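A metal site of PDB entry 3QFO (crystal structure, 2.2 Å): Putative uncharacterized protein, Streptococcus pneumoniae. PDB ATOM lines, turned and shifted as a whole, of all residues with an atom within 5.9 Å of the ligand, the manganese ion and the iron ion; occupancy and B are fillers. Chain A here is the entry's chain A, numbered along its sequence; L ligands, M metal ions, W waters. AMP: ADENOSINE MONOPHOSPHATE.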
ATOM      1  N   ASP A  19      -8.851  13.528  26.457  1.00  0.00           N
ATOM      2  CA  ASP A  19     -10.217  14.025  26.240  1.00  0.00           C
ATOM      3  C   ASP A  19     -10.875  13.322  25.040  1.00  0.00           C
ATOM      4  O   ASP A  19     -11.357  13.964  24.095  1.00  0.00           O
ATOM      5  CB  ASP A  19     -10.185  15.549  26.070  1.00  0.00           C
ATOM      6  CG  ASP A  19      -9.696  16.270  27.330  1.00  0.00           C
ATOM      7  OD1 ASP A  19      -8.572  16.850  27.312  1.00  0.00           O
ATOM      8  OD2 ASP A  19     -10.447  16.227  28.343  1.00  0.00           O
ATOM      9  N   HIS A  21     -13.524  11.295  25.485  1.00  0.00           N
ATOM     10  CA  HIS A  21     -14.936  11.488  25.799  1.00  0.00           C
ATOM     11  C   HIS A  21     -15.855  10.514  25.074  1.00  0.00           C
ATOM     12  O   HIS A  21     -16.915  10.898  24.591  1.00  0.00           O
ATOM     13  CB  HIS A  21     -15.354  12.930  25.510  1.00  0.00           C
ATOM     14  CG  HIS A  21     -14.866  13.916  26.531  1.00  0.00           C
ATOM     15  ND1 HIS A  21     -15.526  14.142  27.721  1.00  0.00           N
ATOM     16  CD2 HIS A  21     -13.771  14.715  26.538  1.00  0.00           C
ATOM     17  CE1 HIS A  21     -14.875  15.059  28.413  1.00  0.00           C
ATOM     18  NE2 HIS A  21     -13.801  15.411  27.726  1.00  0.00           N
ATOM     19  N   GLY A  46      -6.562  11.534  30.308  1.00  0.00           N
ATOM     20  CA  GLY A  46      -7.873  11.424  30.971  1.00  0.00           C
ATOM     21  C   GLY A  46      -9.059  12.016  30.216  1.00  0.00           C
ATOM     22  O   GLY A  46      -8.904  12.568  29.099  1.00  0.00           O
ATOM     23  N   ASP A  47     -10.231  11.928  30.845  1.00  0.00           N
ATOM     24  CA  ASP A  47     -11.539  12.142  30.203  1.00  0.00           C
ATOM     25  C   ASP A  47     -11.723  11.143  29.064  1.00  0.00           C
ATOM     26  O   ASP A  47     -11.777  11.479  27.883  1.00  0.00           O
ATOM     27  CB  ASP A  47     -11.765  13.602  29.786  1.00  0.00           C
ATOM     28  CG  ASP A  47     -11.971  14.529  30.977  1.00  0.00           C
ATOM     29  OD1 ASP A  47     -11.931  14.034  32.133  1.00  0.00           O
ATOM     30  OD2 ASP A  47     -12.154  15.753  30.793  1.00  0.00           O
ATOM     31  N   GLY A  73      -8.656  12.202  34.840  1.00  0.00           N
ATOM     32  CA  GLY A  73      -9.459  13.343  34.405  1.00  0.00           C
ATOM     33  C   GLY A  73     -10.684  13.530  35.288  1.00  0.00           C
ATOM     34  O   GLY A  73     -11.083  12.614  35.999  1.00  0.00           O
ATOM     35  N   ASN A  74     -11.294  14.717  35.239  1.00  0.00           N
ATOM     36  CA  ASN A  74     -12.490  14.978  36.052  1.00  0.00           C
ATOM     37  C   ASN A  74     -13.720  14.144  35.651  1.00  0.00           C
ATOM     38  O   ASN A  74     -14.602  13.913  36.488  1.00  0.00           O
ATOM     39  CB  ASN A  74     -12.829  16.454  36.023  1.00  0.00           C
ATOM     40  CG  ASN A  74     -12.919  16.995  34.601  1.00  0.00           C
ATOM     41  OD1 ASN A  74     -12.070  16.696  33.769  1.00  0.00           O
ATOM     42  ND2 ASN A  74     -13.963  17.747  34.321  1.00  0.00           N
ATOM     43  N   TRP A  75     -13.786  13.704  34.390  1.00  0.00           N
ATOM     44  CA  TRP A  75     -14.884  12.843  33.945  1.00  0.00           C
ATOM     45  C   TRP A  75     -14.799  11.405  34.490  1.00  0.00           C
ATOM     46  O   TRP A  75     -15.817  10.720  34.570  1.00  0.00           O
ATOM     47  CB  TRP A  75     -15.067  12.870  32.423  1.00  0.00           C
ATOM     48  CG  TRP A  75     -15.771  14.124  31.941  1.00  0.00           C
ATOM     49  CD1 TRP A  75     -15.271  15.395  31.955  1.00  0.00           C
ATOM     50  CD2 TRP A  75     -17.083  14.233  31.384  1.00  0.00           C
ATOM     51  NE1 TRP A  75     -16.191  16.290  31.469  1.00  0.00           N
ATOM     52  CE2 TRP A  75     -17.309  15.595  31.089  1.00  0.00           C
ATOM     53  CE3 TRP A  75     -18.106  13.311  31.107  1.00  0.00           C
ATOM     54  CZ2 TRP A  75     -18.510  16.064  30.532  1.00  0.00           C
ATOM     55  CZ3 TRP A  75     -19.315  13.779  30.556  1.00  0.00           C
ATOM     56  CH2 TRP A  75     -19.499  15.141  30.266  1.00  0.00           C
ATOM     57  N   HIS A 136      -4.051  16.090  34.214  1.00  0.00           N
ATOM     58  CA  HIS A 136      -5.217  16.425  33.388  1.00  0.00           C
ATOM     59  C   HIS A 136      -5.371  17.935  33.289  1.00  0.00           C
ATOM     60  O   HIS A 136      -5.511  18.485  32.204  1.00  0.00           O
ATOM     61  CB  HIS A 136      -6.512  15.813  33.928  1.00  0.00           C
ATOM     62  CG  HIS A 136      -7.708  16.052  33.043  1.00  0.00           C
ATOM     63  ND1 HIS A 136      -7.820  15.470  31.796  1.00  0.00           N
ATOM     64  CD2 HIS A 136      -8.823  16.804  33.218  1.00  0.00           C
ATOM     65  CE1 HIS A 136      -8.965  15.849  31.239  1.00  0.00           C
ATOM     66  NE2 HIS A 136      -9.591  16.647  32.091  1.00  0.00           N
ATOM     67  N   ASN A 142      -8.194  18.377  39.025  1.00  0.00           N
ATOM     68  CA  ASN A 142      -8.401  17.976  37.622  1.00  0.00           C
ATOM     69  C   ASN A 142      -9.646  18.602  36.956  1.00  0.00           C
ATOM     70  O   ASN A 142     -10.074  18.170  35.884  1.00  0.00           O
ATOM     71  CB  ASN A 142      -8.408  16.451  37.489  1.00  0.00           C
ATOM     72  CG  ASN A 142      -9.608  15.811  38.144  1.00  0.00           C
ATOM     73  OD1 ASN A 142     -10.545  16.477  38.569  1.00  0.00           O
ATOM     74  ND2 ASN A 142      -9.606  14.494  38.211  1.00  0.00           N
ATOM     75  N   ARG A 145     -11.334  25.999  35.559  1.00  0.00           N
ATOM     76  CA  ARG A 145     -11.067  26.854  34.410  1.00  0.00           C
ATOM     77  C   ARG A 145      -9.784  27.641  34.586  1.00  0.00           C
ATOM     78  O   ARG A 145      -9.528  28.572  33.810  1.00  0.00           O
ATOM     79  CB  ARG A 145     -12.202  27.851  34.207  1.00  0.00           C
ATOM     80  CG  ARG A 145     -13.561  27.262  33.900  1.00  0.00           C
ATOM     81  CD  ARG A 145     -13.557  26.359  32.667  1.00  0.00           C
ATOM     82  NE  ARG A 145     -14.854  26.425  31.981  1.00  0.00           N
ATOM     83  CZ  ARG A 145     -15.493  25.375  31.488  1.00  0.00           C
ATOM     84  NH1 ARG A 145     -16.672  25.546  30.893  1.00  0.00           N
ATOM     85  NH2 ARG A 145     -14.977  24.154  31.609  1.00  0.00           N
ATOM     86  N   ILE A 148      -7.400  27.879  31.254  1.00  0.00           N
ATOM     87  CA  ILE A 148      -7.968  28.223  29.960  1.00  0.00           C
ATOM     88  C   ILE A 148      -6.983  29.084  29.146  1.00  0.00           C
ATOM     89  O   ILE A 148      -5.948  29.529  29.679  1.00  0.00           O
ATOM     90  CB  ILE A 148      -9.339  28.950  30.070  1.00  0.00           C
ATOM     91  CG1 ILE A 148      -9.233  30.240  30.905  1.00  0.00           C
ATOM     92  CG2 ILE A 148     -10.400  27.977  30.591  1.00  0.00           C
ATOM     93  CD1 ILE A 148     -10.534  31.094  30.903  1.00  0.00           C
ATOM     94  N   HIS A 149      -7.313  29.326  27.885  1.00  0.00           N
ATOM     95  CA  HIS A 149      -6.439  30.064  26.972  1.00  0.00           C
ATOM     96  C   HIS A 149      -5.983  31.420  27.529  1.00  0.00           C
ATOM     97  O   HIS A 149      -4.875  31.856  27.257  1.00  0.00           O
ATOM     98  CB  HIS A 149      -7.075  30.195  25.564  1.00  0.00           C
ATOM     99  CG  HIS A 149      -8.246  31.124  25.488  1.00  0.00           C
ATOM    100  ND1 HIS A 149      -9.303  31.069  26.374  1.00  0.00           N
ATOM    101  CD2 HIS A 149      -8.535  32.131  24.630  1.00  0.00           C
ATOM    102  CE1 HIS A 149     -10.180  32.012  26.075  1.00  0.00           C
ATOM    103  NE2 HIS A 149      -9.739  32.670  25.017  1.00  0.00           N
ATOM    104  N   THR A 150      -6.832  32.062  28.332  1.00  0.00           N
ATOM    105  CA  THR A 150      -6.507  33.367  28.914  1.00  0.00           C
ATOM    106  C   THR A 150      -6.179  33.291  30.406  1.00  0.00           C
ATOM    107  O   THR A 150      -6.217  34.309  31.108  1.00  0.00           O
ATOM    108  CB  THR A 150      -7.647  34.386  28.690  1.00  0.00           C
ATOM    109  OG1 THR A 150      -8.890  33.812  29.088  1.00  0.00           O
ATOM    110  CG2 THR A 150      -7.740  34.790  27.223  1.00  0.00           C
ATOM    111  N   HIS A 172      -7.685  18.764  29.319  1.00  0.00           N
ATOM    112  CA  HIS A 172      -8.819  19.425  29.993  1.00  0.00           C
ATOM    113  C   HIS A 172      -9.468  20.605  29.256  1.00  0.00           C
ATOM    114  O   HIS A 172     -10.686  20.757  29.282  1.00  0.00           O
ATOM    115  CB  HIS A 172      -8.459  19.814  31.425  1.00  0.00           C
ATOM    116  CG  HIS A 172      -9.601  20.336  32.225  1.00  0.00           C
ATOM    117  ND1 HIS A 172     -10.727  19.579  32.517  1.00  0.00           N
ATOM    118  CD2 HIS A 172      -9.813  21.565  32.771  1.00  0.00           C
ATOM    119  CE1 HIS A 172     -11.566  20.317  33.228  1.00  0.00           C
ATOM    120  NE2 HIS A 172     -11.040  21.507  33.396  1.00  0.00           N
ATOM    121  N   ILE A 173      -8.667  21.465  28.628  1.00  0.00           N
ATOM    122  CA  ILE A 173      -9.253  22.631  27.968  1.00  0.00           C
ATOM    123  C   ILE A 173      -9.674  22.374  26.516  1.00  0.00           C
ATOM    124  O   ILE A 173     -10.348  23.215  25.918  1.00  0.00           O
ATOM    125  CB  ILE A 173      -8.349  23.885  28.068  1.00  0.00           C
ATOM    126  CG1 ILE A 173      -7.030  23.681  27.301  1.00  0.00           C
ATOM    127  CG2 ILE A 173      -8.128  24.272  29.535  1.00  0.00           C
ATOM    128  CD1 ILE A 173      -6.294  24.982  26.986  1.00  0.00           C
ATOM    129  N   HIS A 174      -9.290  21.216  25.964  1.00  0.00           N
ATOM    130  CA  HIS A 174      -9.741  20.790  24.640  1.00  0.00           C
ATOM    131  C   HIS A 174      -9.201  21.720  23.547  1.00  0.00           C
ATOM    132  O   HIS A 174      -9.840  21.938  22.507  1.00  0.00           O
ATOM    133  CB  HIS A 174     -11.285  20.717  24.581  1.00  0.00           C
ATOM    134  CG  HIS A 174     -11.881  19.594  25.386  1.00  0.00           C
ATOM    135  ND1 HIS A 174     -12.993  18.882  24.963  1.00  0.00           N
ATOM    136  CD2 HIS A 174     -11.509  19.037  26.567  1.00  0.00           C
ATOM    137  CE1 HIS A 174     -13.276  17.944  25.849  1.00  0.00           C
ATOM    138  NE2 HIS A 174     -12.408  18.020  26.839  1.00  0.00           N
ATOM    139  N   GLN A 175      -8.022  22.282  23.804  1.00  0.00           N
ATOM    140  CA  GLN A 175      -7.319  23.134  22.844  1.00  0.00           C
ATOM    141  C   GLN A 175      -5.838  22.753  22.796  1.00  0.00           C
ATOM    142  O   GLN A 175      -5.240  22.437  23.811  1.00  0.00           O
ATOM    143  CB  GLN A 175      -7.414  24.611  23.248  1.00  0.00           C
ATOM    144  CG  GLN A 175      -8.820  25.220  23.340  1.00  0.00           C
ATOM    145  CD  GLN A 175      -8.722  26.728  23.411  1.00  0.00           C
ATOM    146  OE1 GLN A 175      -8.557  27.290  24.498  1.00  0.00           O
ATOM    147  NE2 GLN A 175      -8.717  27.384  22.242  1.00  0.00           N
ATOM    148  N   SER A 192      -8.165  17.886  22.205  1.00  0.00           N
ATOM    149  CA  SER A 192      -9.122  16.808  22.481  1.00  0.00           C
ATOM    150  C   SER A 192      -9.333  15.904  21.267  1.00  0.00           C
ATOM    151  O   SER A 192      -9.572  16.365  20.166  1.00  0.00           O
ATOM    152  CB  SER A 192     -10.471  17.435  22.901  1.00  0.00           C
ATOM    153  OG  SER A 192     -11.478  16.455  23.057  1.00  0.00           O
ATOM    154  N   GLN A 195     -13.802  15.817  21.351  1.00  0.00           N
ATOM    155  CA  GLN A 195     -14.609  17.019  21.539  1.00  0.00           C
ATOM    156  C   GLN A 195     -13.751  18.293  21.343  1.00  0.00           C
ATOM    157  O   GLN A 195     -13.693  19.127  22.250  1.00  0.00           O
ATOM    158  CB  GLN A 195     -15.224  17.081  22.951  1.00  0.00           C
ATOM    159  CG  GLN A 195     -16.129  15.902  23.398  1.00  0.00           C
ATOM    160  CD  GLN A 195     -17.528  15.974  22.793  1.00  0.00           C
ATOM    161  OE1 GLN A 195     -18.479  16.404  23.458  1.00  0.00           O
ATOM    162  NE2 GLN A 195     -17.651  15.583  21.529  1.00  0.00           N
ATOM    163  N   PHE A 197     -12.293  21.932  20.792  1.00  0.00           N
ATOM    164  CA  PHE A 197     -12.963  23.138  21.231  1.00  0.00           C
ATOM    165  C   PHE A 197     -12.313  24.375  20.660  1.00  0.00           C
ATOM    166  O   PHE A 197     -11.101  24.576  20.777  1.00  0.00           O
ATOM    167  CB  PHE A 197     -13.050  23.211  22.758  1.00  0.00           C
ATOM    168  CG  PHE A 197     -13.721  24.452  23.277  1.00  0.00           C
ATOM    169  CD1 PHE A 197     -15.101  24.646  23.103  1.00  0.00           C
ATOM    170  CD2 PHE A 197     -12.979  25.441  23.927  1.00  0.00           C
ATOM    171  CE1 PHE A 197     -15.738  25.821  23.564  1.00  0.00           C
ATOM    172  CE2 PHE A 197     -13.603  26.615  24.403  1.00  0.00           C
ATOM    173  CZ  PHE A 197     -14.982  26.800  24.215  1.00  0.00           C
ATOM    174  N   LEU A 199     -12.978  28.685  20.191  1.00  0.00           N
ATOM    175  CA  LEU A 199     -13.726  29.914  20.437  1.00  0.00           C
ATOM    176  C   LEU A 199     -13.870  30.708  19.139  1.00  0.00           C
ATOM    177  O   LEU A 199     -14.758  31.550  19.010  1.00  0.00           O
ATOM    178  CB  LEU A 199     -13.075  30.785  21.526  1.00  0.00           C
ATOM    179  CG  LEU A 199     -13.265  30.332  22.973  1.00  0.00           C
ATOM    180  CD1 LEU A 199     -12.115  29.453  23.378  1.00  0.00           C
ATOM    181  CD2 LEU A 199     -13.315  31.514  23.926  1.00  0.00           C
ATOM    182  N   HIS A 260     -20.683  23.661  22.545  1.00  0.00           N
ATOM    183  CA  HIS A 260     -20.763  22.804  23.736  1.00  0.00           C
ATOM    184  C   HIS A 260     -21.834  23.264  24.732  1.00  0.00           C
ATOM    185  O   HIS A 260     -21.786  24.394  25.230  1.00  0.00           O
ATOM    186  CB  HIS A 260     -19.386  22.668  24.406  1.00  0.00           C
ATOM    187  CG  HIS A 260     -18.355  21.948  23.567  1.00  0.00           C
ATOM    188  ND1 HIS A 260     -17.019  21.924  23.904  1.00  0.00           N
ATOM    189  CD2 HIS A 260     -18.473  21.239  22.433  1.00  0.00           C
ATOM    190  CE1 HIS A 260     -16.359  21.218  23.005  1.00  0.00           C
ATOM    191  NE2 HIS A 260     -17.218  20.787  22.099  1.00  0.00           N
HETATM  192  P   AMP L   1     -14.230  18.897  30.587  1.00  0.00           P
HETATM  193  O1P AMP L   1     -13.320  18.591  31.751  1.00  0.00           O
HETATM  194  O2P AMP L   1     -14.089  17.970  29.411  1.00  0.00           O
HETATM  195  O3P AMP L   1     -15.651  19.051  31.048  1.00  0.00           O
HETATM  196  O5' AMP L   1     -13.786  20.370  30.095  1.00  0.00           O
HETATM  197  C5' AMP L   1     -13.564  20.707  28.730  1.00  0.00           C
HETATM  198  C4' AMP L   1     -14.577  21.742  28.250  1.00  0.00           C
HETATM  199  O4' AMP L   1     -14.431  23.003  28.909  1.00  0.00           O
HETATM  200  C3' AMP L   1     -14.378  22.096  26.776  1.00  0.00           C
HETATM  201  O3' AMP L   1     -14.967  21.131  25.902  1.00  0.00           O
HETATM  202  C2' AMP L   1     -15.086  23.418  26.661  1.00  0.00           C
HETATM  203  O2' AMP L   1     -16.480  23.198  26.381  1.00  0.00           O
HETATM  204  C1' AMP L   1     -14.888  24.041  28.034  1.00  0.00           C
HETATM  205  N9  AMP L   1     -13.895  25.141  27.884  1.00  0.00           N
HETATM  206  C8  AMP L   1     -12.551  25.007  27.745  1.00  0.00           C
HETATM  207  N7  AMP L   1     -11.957  26.226  27.616  1.00  0.00           N
HETATM  208  C5  AMP L   1     -12.929  27.156  27.676  1.00  0.00           C
HETATM  209  C6  AMP L   1     -12.992  28.635  27.592  1.00  0.00           C
HETATM  210  N6  AMP L   1     -11.865  29.364  27.426  1.00  0.00           N
HETATM  211  N1  AMP L   1     -14.220  29.223  27.680  1.00  0.00           N
HETATM  212  C2  AMP L   1     -15.359  28.514  27.832  1.00  0.00           C
HETATM  213  N3  AMP L   1     -15.367  27.156  27.916  1.00  0.00           N
HETATM  214  C4  AMP L   1     -14.206  26.437  27.847  1.00  0.00           C
HETATM  215 MN    MN M   1     -11.511  17.570  31.833  1.00  0.00          MN
HETATM  216 FE    FE M   2     -12.423  16.838  28.715  1.00  0.00          FE
HETATM  217  O   HOH W   1     -16.301  18.396  27.350  1.00  0.00           O
HETATM  218  O   HOH W   2      -9.608  27.534  26.993  1.00  0.00           O
HETATM  219  O   HOH W   3     -11.813  18.346  30.032  1.00  0.00           O
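Water W3 is bound to the iron ion, 2.1 Å away. The iron ion is bound by OD2 of Asp 19 (2.1 Å). An oxygen (O2P) of the ligand is bound to the iron ion (2.1 Å). NE2 of His 21 binds the iron ion (2.2 Å). The iron ion is bound by a ring nitrogen (NE2) of His 174 (2.2 Å). The side-chain carboxylate (OD2) of Asp 47 binds the iron ion, at 2.4 Å.
Five residues have an atom within 4 Å of the manganese ion: Asp 19, Asp 47, Asn 74, His 136 and His 172. The nearest printed residue that does not touch the manganese ion is Asn 142 (4.3 Å).
The manganese ion is bound by water W3, at 2.0 Å. The manganese ion is bound by O1P of the ligand. The manganese ion is bound by NE2 of His 136. The side-chain carboxylate (OD2) of Asp 47 is bound to the manganese ion, at 2.2 Å. The manganese ion is bound by OD1 of Asn 74 (2.2 Å). A ring nitrogen (ND1) of His 172 is bound to the manganese ion, 2.3 Å away.
A ring nitrogen (ND1) of His 260 is in hydrogen-bond range of an oxygen (O2') of the ligand (2.8 Å). An oxygen (O3P) of the ligand lies within hydrogen-bond range of the indole nitrogen of Trp 75. An oxygen (O4') of the ligand sits at hydrogen-bond distance from the guanidinium group of Arg 145 (3.0 Å). ND1 of His 149 sits at hydrogen-bond distance from N6 of the ligand (3.3 Å).
Water W3 lies within hydrogen-bond range of the backbone carbonyl oxygen (O) of His 172 (2.8 Å) and an oxygen (O5') of the ligand (2.8 Å). Water W2 lies within hydrogen-bond range of the side-chain amide oxygen of Gln 175 (2.7 Å), a nitrogen (N7) of the ligand (2.8 Å) and the backbone NH of His 149 (3.0 Å).
The backbone NH (N) of His 172 sits at hydrogen-bond distance from the side-chain carboxylate (OD1) of Asp 19 (2.9 Å). The backbone NH (N) of Asp 19 sits at hydrogen-bond distance from the backbone carbonyl oxygen (O) of Gly 46 (2.8 Å). The backbone carbonyl oxygen (O) of Asp 19 is in hydrogen-bond range of the side-chain hydroxyl (OG) of Ser 192 (2.7 Å). N of Trp 75 is in hydrogen-bond range of OD1 of Asp 47. The backbone NH (N) of Asn 74 lies close to the side-chain amide nitrogen (ND2) of Asn 142, at 3.4 Å. The backbone carbonyl oxygen (O) of His 174 sits at hydrogen-bond distance from the backbone NH (N) of Phe 197. O of Gln 195 lies within hydrogen-bond range of ND1 of His 174 (2.8 Å). The side-chain hydroxyl of Ser 192 sits at hydrogen-bond distance from a ring nitrogen (ND1) of His 174, 3.4 Å away.
Within 4 Å of the iron ion: Asp 19, His 21, Asp 47 and His 174. The nearest printed residue that does not touch the iron ion is His 172 (4.3 Å).
Residues that only touch the ligand: Ile 148, Ile 173 and Phe 197. Hydrophobic or aromatic side chains that line the ligand: His 21, Trp 75, Ile 148, His 149, His 172, His 174, Phe 197 and His 260. 12 residues have an atom within 4 Å of the ligand: His 21, Asp 47, Asn 74, Trp 75, Arg 145, Ile 148, His 149, His 172, Ile 173, His 174, Phe 197 and His 260. The nearest printed residue that does not touch the ligand is Leu 199 (4.1 Å).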
